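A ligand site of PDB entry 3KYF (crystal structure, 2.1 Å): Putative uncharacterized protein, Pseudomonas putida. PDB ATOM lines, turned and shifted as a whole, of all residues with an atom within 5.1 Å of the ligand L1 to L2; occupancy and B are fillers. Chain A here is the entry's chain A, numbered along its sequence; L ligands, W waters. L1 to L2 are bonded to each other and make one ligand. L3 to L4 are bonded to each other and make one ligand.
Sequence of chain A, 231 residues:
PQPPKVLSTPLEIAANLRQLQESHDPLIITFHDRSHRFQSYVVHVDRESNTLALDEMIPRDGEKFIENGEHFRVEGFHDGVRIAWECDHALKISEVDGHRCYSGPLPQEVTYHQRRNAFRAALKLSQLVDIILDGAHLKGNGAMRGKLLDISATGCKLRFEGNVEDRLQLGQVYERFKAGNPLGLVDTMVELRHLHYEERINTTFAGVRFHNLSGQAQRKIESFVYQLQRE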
ATOM      1  N   PHE A  77     -19.837 -25.971   2.782  1.00  0.00           N
ATOM      2  CA  PHE A  77     -18.770 -25.563   1.888  1.00  0.00           C
ATOM      3  C   PHE A  77     -17.432 -26.178   2.239  1.00  0.00           C
ATOM      4  O   PHE A  77     -17.074 -26.299   3.404  1.00  0.00           O
ATOM      5  CB  PHE A  77     -18.604 -24.046   1.872  1.00  0.00           C
ATOM      6  CG  PHE A  77     -19.638 -23.330   1.073  1.00  0.00           C
ATOM      7  CD1 PHE A  77     -20.913 -23.107   1.597  1.00  0.00           C
ATOM      8  CD2 PHE A  77     -19.365 -22.918  -0.224  1.00  0.00           C
ATOM      9  CE1 PHE A  77     -21.898 -22.482   0.836  1.00  0.00           C
ATOM     10  CE2 PHE A  77     -20.341 -22.290  -1.005  1.00  0.00           C
ATOM     11  CZ  PHE A  77     -21.608 -22.077  -0.474  1.00  0.00           C
ATOM     12  N   GLY A  80     -14.409 -23.550  -0.806  1.00  0.00           N
ATOM     13  CA  GLY A  80     -15.211 -22.765  -1.729  1.00  0.00           C
ATOM     14  C   GLY A  80     -16.330 -23.488  -2.474  1.00  0.00           C
ATOM     15  O   GLY A  80     -17.212 -22.825  -3.026  1.00  0.00           O
ATOM     16  N   VAL A  81     -16.275 -24.821  -2.507  1.00  0.00           N
ATOM     17  CA  VAL A  81     -17.283 -25.642  -3.205  1.00  0.00           C
ATOM     18  C   VAL A  81     -18.487 -25.969  -2.326  1.00  0.00           C
ATOM     19  O   VAL A  81     -18.321 -26.407  -1.172  1.00  0.00           O
ATOM     20  CB  VAL A  81     -16.691 -27.001  -3.667  1.00  0.00           C
ATOM     21  CG1 VAL A  81     -17.712 -27.763  -4.504  1.00  0.00           C
ATOM     22  CG2 VAL A  81     -15.416 -26.772  -4.459  1.00  0.00           C
ATOM     23  N   ARG A  82     -19.684 -25.765  -2.860  1.00  0.00           N
ATOM     24  CA  ARG A  82     -20.878 -26.083  -2.099  1.00  0.00           C
ATOM     25  C   ARG A  82     -21.178 -27.555  -2.318  1.00  0.00           C
ATOM     26  O   ARG A  82     -21.448 -27.976  -3.455  1.00  0.00           O
ATOM     27  CB  ARG A  82     -22.087 -25.253  -2.543  1.00  0.00           C
ATOM     28  CG  ARG A  82     -23.333 -25.530  -1.693  1.00  0.00           C
ATOM     29  CD  ARG A  82     -24.627 -24.975  -2.282  1.00  0.00           C
ATOM     30  NE  ARG A  82     -24.764 -23.539  -2.118  1.00  0.00           N
ATOM     31  CZ  ARG A  82     -24.617 -22.636  -3.095  1.00  0.00           C
ATOM     32  NH1 ARG A  82     -24.311 -23.026  -4.335  1.00  0.00           N
ATOM     33  NH2 ARG A  82     -24.787 -21.352  -2.833  1.00  0.00           N
ATOM     34  N   HIS A 113     -20.874 -27.748  -6.438  1.00  0.00           N
ATOM     35  CA  HIS A 113     -21.012 -26.490  -7.156  1.00  0.00           C
ATOM     36  C   HIS A 113     -20.086 -25.354  -6.692  1.00  0.00           C
ATOM     37  O   HIS A 113     -20.056 -24.986  -5.513  1.00  0.00           O
ATOM     38  CB  HIS A 113     -22.464 -26.036  -6.992  1.00  0.00           C
ATOM     39  CG  HIS A 113     -22.989 -25.214  -8.136  1.00  0.00           C
ATOM     40  ND1 HIS A 113     -24.058 -24.357  -7.995  1.00  0.00           N
ATOM     41  CD2 HIS A 113     -22.632 -25.175  -9.445  1.00  0.00           C
ATOM     42  CE1 HIS A 113     -24.349 -23.819  -9.168  1.00  0.00           C
ATOM     43  NE2 HIS A 113     -23.507 -24.300 -10.063  1.00  0.00           N
ATOM     44  N   GLN A 114     -19.317 -24.806  -7.631  1.00  0.00           N
ATOM     45  CA  GLN A 114     -18.423 -23.691  -7.361  1.00  0.00           C
ATOM     46  C   GLN A 114     -18.632 -22.791  -8.595  1.00  0.00           C
ATOM     47  O   GLN A 114     -18.182 -23.110  -9.694  1.00  0.00           O
ATOM     48  CB  GLN A 114     -16.980 -24.181  -7.241  1.00  0.00           C
ATOM     49  CG  GLN A 114     -16.045 -23.225  -6.529  1.00  0.00           C
ATOM     50  CD  GLN A 114     -15.921 -21.880  -7.247  1.00  0.00           C
ATOM     51  OE1 GLN A 114     -16.637 -20.923  -6.940  1.00  0.00           O
ATOM     52  NE2 GLN A 114     -15.034 -21.827  -8.223  1.00  0.00           N
ATOM     53  N   ARG A 115     -19.318 -21.668  -8.382  1.00  0.00           N
ATOM     54  CA  ARG A 115     -19.688 -20.738  -9.454  1.00  0.00           C
ATOM     55  C   ARG A 115     -18.698 -19.677  -9.946  1.00  0.00           C
ATOM     56  O   ARG A 115     -18.942 -19.086 -10.979  1.00  0.00           O
ATOM     57  CB  ARG A 115     -20.974 -20.021  -9.056  1.00  0.00           C
ATOM     58  CG  ARG A 115     -22.107 -20.982  -8.709  1.00  0.00           C
ATOM     59  CD  ARG A 115     -23.316 -20.271  -8.143  1.00  0.00           C
ATOM     60  NE  ARG A 115     -23.066 -19.837  -6.772  1.00  0.00           N
ATOM     61  CZ  ARG A 115     -23.972 -19.275  -5.978  1.00  0.00           C
ATOM     62  NH1 ARG A 115     -25.208 -19.088  -6.427  1.00  0.00           N
ATOM     63  NH2 ARG A 115     -23.649 -18.945  -4.741  1.00  0.00           N
ATOM     64  N   ARG A 116     -17.607 -19.433  -9.231  1.00  0.00           N
ATOM     65  CA  ARG A 116     -16.653 -18.402  -9.643  1.00  0.00           C
ATOM     66  C   ARG A 116     -15.567 -18.877 -10.594  1.00  0.00           C
ATOM     67  O   ARG A 116     -14.927 -19.910 -10.370  1.00  0.00           O
ATOM     68  CB  ARG A 116     -15.994 -17.790  -8.399  1.00  0.00           C
ATOM     69  CG  ARG A 116     -16.999 -17.373  -7.338  1.00  0.00           C
ATOM     70  CD  ARG A 116     -16.320 -17.003  -6.039  1.00  0.00           C
ATOM     71  NE  ARG A 116     -17.292 -16.519  -5.075  1.00  0.00           N
ATOM     72  CZ  ARG A 116     -17.012 -16.119  -3.842  1.00  0.00           C
ATOM     73  NH1 ARG A 116     -15.751 -16.152  -3.401  1.00  0.00           N
ATOM     74  NH2 ARG A 116     -17.974 -15.683  -3.065  1.00  0.00           N
ATOM     75  N   ARG A 120     -11.050 -15.375  -5.554  1.00  0.00           N
ATOM     76  CA  ARG A 120     -11.090 -14.028  -4.999  1.00  0.00           C
ATOM     77  C   ARG A 120     -10.195 -13.940  -3.761  1.00  0.00           C
ATOM     78  O   ARG A 120     -10.434 -14.632  -2.776  1.00  0.00           O
ATOM     79  CB  ARG A 120     -12.532 -13.657  -4.616  1.00  0.00           C
ATOM     80  CG  ARG A 120     -13.485 -13.653  -5.802  1.00  0.00           C
ATOM     81  CD  ARG A 120     -14.922 -13.364  -5.405  1.00  0.00           C
ATOM     82  NE  ARG A 120     -15.828 -13.523  -6.546  1.00  0.00           N
ATOM     83  CZ  ARG A 120     -17.146 -13.352  -6.481  1.00  0.00           C
ATOM     84  NH1 ARG A 120     -17.724 -13.019  -5.342  1.00  0.00           N
ATOM     85  NH2 ARG A 120     -17.887 -13.554  -7.551  1.00  0.00           N
ATOM     86  N   LYS A 157     -14.509  -6.725  -5.123  1.00  0.00           N
ATOM     87  CA  LYS A 157     -15.524  -6.311  -4.160  1.00  0.00           C
ATOM     88  C   LYS A 157     -15.110  -4.932  -3.612  1.00  0.00           C
ATOM     89  O   LYS A 157     -13.950  -4.719  -3.218  1.00  0.00           O
ATOM     90  CB  LYS A 157     -15.619  -7.320  -3.007  1.00  0.00           C
ATOM     91  CG  LYS A 157     -16.740  -7.001  -2.028  1.00  0.00           C
ATOM     92  CD  LYS A 157     -16.744  -7.954  -0.857  1.00  0.00           C
ATOM     93  CE  LYS A 157     -16.945  -9.399  -1.315  1.00  0.00           C
ATOM     94  NZ  LYS A 157     -18.258  -9.618  -2.001  1.00  0.00           N
ATOM     95  N   ARG A 193     -22.494  -5.674 -10.415  1.00  0.00           N
ATOM     96  CA  ARG A 193     -23.169  -6.975 -10.419  1.00  0.00           C
ATOM     97  C   ARG A 193     -24.092  -7.200  -9.219  1.00  0.00           C
ATOM     98  O   ARG A 193     -25.114  -7.883  -9.333  1.00  0.00           O
ATOM     99  CB  ARG A 193     -22.127  -8.088 -10.473  1.00  0.00           C
ATOM    100  CG  ARG A 193     -21.321  -8.109 -11.751  1.00  0.00           C
ATOM    101  CD  ARG A 193     -22.124  -8.774 -12.849  1.00  0.00           C
ATOM    102  NE  ARG A 193     -23.266  -7.979 -13.270  1.00  0.00           N
ATOM    103  CZ  ARG A 193     -24.390  -8.493 -13.765  1.00  0.00           C
ATOM    104  NH1 ARG A 193     -24.536  -9.805 -13.889  1.00  0.00           N
ATOM    105  NH2 ARG A 193     -25.362  -7.688 -14.172  1.00  0.00           N
ATOM    106  N   HIS A 194     -23.704  -6.635  -8.079  1.00  0.00           N
ATOM    107  CA  HIS A 194     -24.497  -6.760  -6.874  1.00  0.00           C
ATOM    108  C   HIS A 194     -24.090  -5.715  -5.852  1.00  0.00           C
ATOM    109  O   HIS A 194     -22.962  -5.217  -5.846  1.00  0.00           O
ATOM    110  CB  HIS A 194     -24.380  -8.176  -6.275  1.00  0.00           C
ATOM    111  CG  HIS A 194     -23.037  -8.487  -5.675  1.00  0.00           C
ATOM    112  ND1 HIS A 194     -22.711  -8.198  -4.373  1.00  0.00           N
ATOM    113  CD2 HIS A 194     -21.934  -9.047  -6.227  1.00  0.00           C
ATOM    114  CE1 HIS A 194     -21.465  -8.571  -4.134  1.00  0.00           C
ATOM    115  NE2 HIS A 194     -20.966  -9.084  -5.244  1.00  0.00           N
HETATM  116  P1  LIG L   1     -18.893 -13.932   0.508  1.00  0.00           P
HETATM  117  O1  LIG L   1     -18.283 -13.030   1.520  1.00  0.00           O
HETATM  118  O2  LIG L   1     -17.972 -14.161  -0.637  1.00  0.00           O
HETATM  119  O3  LIG L   1     -20.211 -13.294  -0.128  1.00  0.00           O
HETATM  120  C1  LIG L   1     -21.211 -12.727   0.728  1.00  0.00           C
HETATM  121  C2  LIG L   1     -22.462 -12.342  -0.074  1.00  0.00           C
HETATM  122  O4  LIG L   1     -22.161 -11.384  -1.099  1.00  0.00           O
HETATM  123  C3  LIG L   1     -23.013 -13.558  -0.828  1.00  0.00           C
HETATM  124  O5  LIG L   1     -23.807 -14.322   0.097  1.00  0.00           O
HETATM  125  C4  LIG L   1     -23.929 -12.811  -1.788  1.00  0.00           C
HETATM  126  O6  LIG L   1     -25.054 -12.282  -1.092  1.00  0.00           O
HETATM  127  C5  LIG L   1     -23.019 -11.663  -2.225  1.00  0.00           C
HETATM  128  N1  LIG L   1     -22.174 -12.084  -3.369  1.00  0.00           N
HETATM  129  C6  LIG L   1     -20.901 -12.473  -3.312  1.00  0.00           C
HETATM  130  N2  LIG L   1     -20.467 -12.751  -4.543  1.00  0.00           N
HETATM  131  C7  LIG L   1     -21.475 -12.541  -5.394  1.00  0.00           C
HETATM  132  C8  LIG L   1     -21.594 -12.641  -6.766  1.00  0.00           C
HETATM  133  O7  LIG L   1     -20.648 -13.012  -7.459  1.00  0.00           O
HETATM  134  N3  LIG L   1     -22.818 -12.316  -7.364  1.00  0.00           N
HETATM  135  C9  LIG L   1     -23.886 -11.892  -6.549  1.00  0.00           C
HETATM  136  N4  LIG L   1     -25.042 -11.541  -7.103  1.00  0.00           N
HETATM  137  N5  LIG L   1     -23.723 -11.795  -5.225  1.00  0.00           N
HETATM  138  C10 LIG L   1     -22.560 -12.104  -4.639  1.00  0.00           C
HETATM  139  P1  LG2 L   2     -24.172 -15.855  -0.172  1.00  0.00           P
HETATM  140  O1  LG2 L   2     -24.660 -16.082  -1.553  1.00  0.00           O
HETATM  141  O2  LG2 L   2     -25.139 -16.345   0.839  1.00  0.00           O
HETATM  142  O3  LG2 L   2     -22.822 -16.671   0.106  1.00  0.00           O
HETATM  143  C1  LG2 L   2     -22.201 -16.629   1.391  1.00  0.00           C
HETATM  144  C2  LG2 L   2     -20.788 -17.218   1.315  1.00  0.00           C
HETATM  145  O4  LG2 L   2     -20.788 -18.528   0.726  1.00  0.00           O
HETATM  146  C3  LG2 L   2     -19.908 -16.370   0.393  1.00  0.00           C
HETATM  147  O5  LG2 L   2     -19.393 -15.297   1.180  1.00  0.00           O
HETATM  148  C4  LG2 L   2     -18.789 -17.368   0.122  1.00  0.00           C
HETATM  149  O6  LG2 L   2     -17.922 -17.475   1.255  1.00  0.00           O
HETATM  150  C5  LG2 L   2     -19.586 -18.667  -0.046  1.00  0.00           C
HETATM  151  N1  LG2 L   2     -19.972 -18.846  -1.459  1.00  0.00           N
HETATM  152  C6  LG2 L   2     -21.203 -18.820  -1.966  1.00  0.00           C
HETATM  153  N2  LG2 L   2     -21.168 -19.178  -3.238  1.00  0.00           N
HETATM  154  C7  LG2 L   2     -19.896 -19.425  -3.564  1.00  0.00           C
HETATM  155  C8  LG2 L   2     -19.275 -19.858  -4.723  1.00  0.00           C
HETATM  156  O7  LG2 L   2     -19.936 -20.157  -5.726  1.00  0.00           O
HETATM  157  N3  LG2 L   2     -17.889 -20.027  -4.722  1.00  0.00           N
HETATM  158  C9  LG2 L   2     -17.159 -19.756  -3.557  1.00  0.00           C
HETATM  159  N4  LG2 L   2     -15.841 -19.870  -3.552  1.00  0.00           N
HETATM  160  N5  LG2 L   2     -17.804 -19.357  -2.441  1.00  0.00           N
HETATM  161  C10 LG2 L   2     -19.128 -19.195  -2.434  1.00  0.00           C
HETATM  162  P1  LG3 L   3     -22.534 -12.150 -11.153  1.00  0.00           P
HETATM  163  O1  LG3 L   3     -23.167 -11.736  -9.873  1.00  0.00           O
HETATM  164  O2  LG3 L   3     -23.197 -11.533 -12.330  1.00  0.00           O
HETATM  165  O3  LG3 L   3     -21.012 -11.676 -11.216  1.00  0.00           O
HETATM  166  C1  LG3 L   3     -20.267 -11.794 -12.431  1.00  0.00           C
HETATM  167  C2  LG3 L   3     -18.800 -11.447 -12.156  1.00  0.00           C
HETATM  168  O4  LG3 L   3     -18.668 -10.188 -11.471  1.00  0.00           O
HETATM  169  C3  LG3 L   3     -18.174 -12.444 -11.185  1.00  0.00           C
HETATM  170  O5  LG3 L   3     -17.876 -13.652 -11.895  1.00  0.00           O
HETATM  171  C4  LG3 L   3     -16.893 -11.658 -10.938  1.00  0.00           C
HETATM  172  O6  LG3 L   3     -16.113 -11.615 -12.137  1.00  0.00           O
HETATM  173  C5  LG3 L   3     -17.471 -10.265 -10.674  1.00  0.00           C
HETATM  174  N1  LG3 L   3     -17.889 -10.095  -9.259  1.00  0.00           N
HETATM  175  C6  LG3 L   3     -19.127  -9.863  -8.841  1.00  0.00           C
HETATM  176  N2  LG3 L   3     -19.118  -9.687  -7.517  1.00  0.00           N
HETATM  177  C7  LG3 L   3     -17.868  -9.813  -7.100  1.00  0.00           C
HETATM  178  C8  LG3 L   3     -17.282  -9.730  -5.836  1.00  0.00           C
HETATM  179  O7  LG3 L   3     -17.948  -9.457  -4.841  1.00  0.00           O
HETATM  180  N3  LG3 L   3     -15.901  -9.935  -5.727  1.00  0.00           N
HETATM  181  C9  LG3 L   3     -15.152 -10.224  -6.878  1.00  0.00           C
HETATM  182  N4  LG3 L   3     -13.847 -10.426  -6.794  1.00  0.00           N
HETATM  183  N5  LG3 L   3     -15.756 -10.281  -8.079  1.00  0.00           N
HETATM  184  C10 LG3 L   3     -17.075 -10.082  -8.204  1.00  0.00           C
HETATM  185  P1  LG4 L   4     -17.729 -15.033 -11.096  1.00  0.00           P
HETATM  186  O1  LG4 L   4     -16.790 -14.922  -9.955  1.00  0.00           O
HETATM  187  O2  LG4 L   4     -17.349 -16.145 -12.011  1.00  0.00           O
HETATM  188  O3  LG4 L   4     -19.200 -15.400 -10.595  1.00  0.00           O
HETATM  189  C1  LG4 L   4     -20.202 -15.788 -11.550  1.00  0.00           C
HETATM  190  C2  LG4 L   4     -21.566 -15.894 -10.877  1.00  0.00           C
HETATM  191  O4  LG4 L   4     -21.562 -16.819  -9.773  1.00  0.00           O
HETATM  192  C3  LG4 L   4     -21.943 -14.559 -10.235  1.00  0.00           C
HETATM  193  O5  LG4 L   4     -22.463 -13.739 -11.293  1.00  0.00           O
HETATM  194  C4  LG4 L   4     -23.083 -15.045  -9.352  1.00  0.00           C
HETATM  195  O6  LG4 L   4     -24.239 -15.303 -10.162  1.00  0.00           O
HETATM  196  C5  LG4 L   4     -22.533 -16.358  -8.811  1.00  0.00           C
HETATM  197  N1  LG4 L   4     -21.797 -16.167  -7.538  1.00  0.00           N
HETATM  198  C6  LG4 L   4     -20.486 -16.222  -7.372  1.00  0.00           C
HETATM  199  N2  LG4 L   4     -20.190 -16.113  -6.076  1.00  0.00           N
HETATM  200  C7  LG4 L   4     -21.338 -15.981  -5.419  1.00  0.00           C
HETATM  201  C8  LG4 L   4     -21.639 -15.842  -4.067  1.00  0.00           C
HETATM  202  O7  LG4 L   4     -20.750 -15.863  -3.223  1.00  0.00           O
HETATM  203  N3  LG4 L   4     -22.987 -15.727  -3.696  1.00  0.00           N
HETATM  204  C9  LG4 L   4     -23.975 -15.753  -4.684  1.00  0.00           C
HETATM  205  N4  LG4 L   4     -25.260 -15.610  -4.354  1.00  0.00           N
HETATM  206  N5  LG4 L   4     -23.647 -15.896  -5.974  1.00  0.00           N
HETATM  207  C10 LG4 L   4     -22.364 -16.013  -6.350  1.00  0.00           C
HETATM  208  O   HOH W   1     -12.663 -20.447  -2.750  1.00  0.00           O
HETATM  209  O   HOH W   2     -16.216 -19.246  -0.386  1.00  0.00           O
HETATM  210  O   HOH W   3     -25.586 -18.429  -2.271  1.00  0.00           O
HETATM  211  O   HOH W   4     -15.478 -14.991  -0.573  1.00  0.00           O
HETATM  212  O   HOH W   5     -25.803 -11.148  -9.838  1.00  0.00           O
HETATM  213  O   HOH W   6     -25.874 -10.729  -3.590  1.00  0.00           O
HETATM  214  O   HOH W   7     -20.700  -8.808  -0.282  1.00  0.00           O
HETATM  215  O   HOH W   8     -20.225 -20.505   3.479  1.00  0.00           O
HETATM  216  O   HOH W   9     -16.671 -12.032  -2.825  1.00  0.00           O
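The guanidinium group of Arg 115 lies close to a nitrogen (N5) of LG4 L4 (3.3 Å).
NZ of Lys 157 sits at hydrogen-bond distance from O7 of LG3 L3 (2.9 Å).
N2 of LG2 L2 is in hydrogen-bond range of NH2 of Arg 115, 2.9 Å away.
The guanidinium group of Arg 116 lies within salt-bridge range of an oxygen (O2) of LIG L1, at 2.9 Å.
An oxygen (O2) of LG3 L3 lies within salt-bridge range of the guanidinium group (NH1) of Arg 193.
NH2 of Arg 116 lies within hydrogen-bond range of O7 of LG4 L4.
OE1 of Gln 114 sits at hydrogen-bond distance from N3 of LG2 L2, 2.7 Å away.
N of Arg 115 is in hydrogen-bond range of O7 of LG2 L2, at 3.1 Å.
A ring nitrogen (NE2) of His 194 lies within hydrogen-bond range of a nitrogen (N2) of LG3 L3, at 3.0 Å.
NH2 of Arg 120 is in hydrogen-bond range of O7 of LIG L1 (2.8 Å).
An oxygen (O1) of LG4 L4 is in salt-bridge range of the guanidinium group (NH2) of Arg 120, at 3.0 Å.
O of Gly 80 lies close to N4 of LG2 L2 (3.3 Å).
The side-chain amide nitrogen of Gln 114 lies within hydrogen-bond range of the backbone carbonyl oxygen of Arg 116, 2.9 Å away.
CE2 of Phe 77 touches N1 of LG2 L2, 3.5 Å away.
CG of His 194 touches N5 of LIG L1, at 3.4 Å.
Hydrophobic or aromatic side chains within 4 Å of the ligand L1 to L2: Phe 77 and His 194.
Of the 12 residues printed, 7 come within 4 Å of the ligand L1 to L2.
The nearest printed residue that does not touch the ligand L1 to L2 is Lys 157 (4.1 Å).
An oxygen (O1) of LG3 L3 lies within hydrogen-bond range of a nitrogen (N3) of LIG L1 (2.6 Å).
Water W3 lies within hydrogen-bond range of an oxygen (O1) of LG2 L2, the guanidinium group of Arg 82 and the guanidinium group of Arg 115.
Water W4 lies within hydrogen-bond range of O2 of LIG L1 (2.6 Å) and NH1 of Arg 116 (3.1 Å).
Water W5 lies within hydrogen-bond range of an oxygen (O1) of LG3 L3 (2.7 Å), a nitrogen (N4) of LIG L1 (2.9 Å) and the backbone carbonyl oxygen of Arg 193 (3.4 Å).
Water W7 lies within hydrogen-bond range of an oxygen (O4) of LIG L1 and the side-chain amino group (NZ) of Lys 157.
Water W9 lies within hydrogen-bond range of the guanidinium group (NH1) of Arg 120 (2.9 Å), the side-chain amino group (NZ) of Lys 157 (3.0 Å) and an oxygen (O2) of LIG L1 (3.3 Å).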
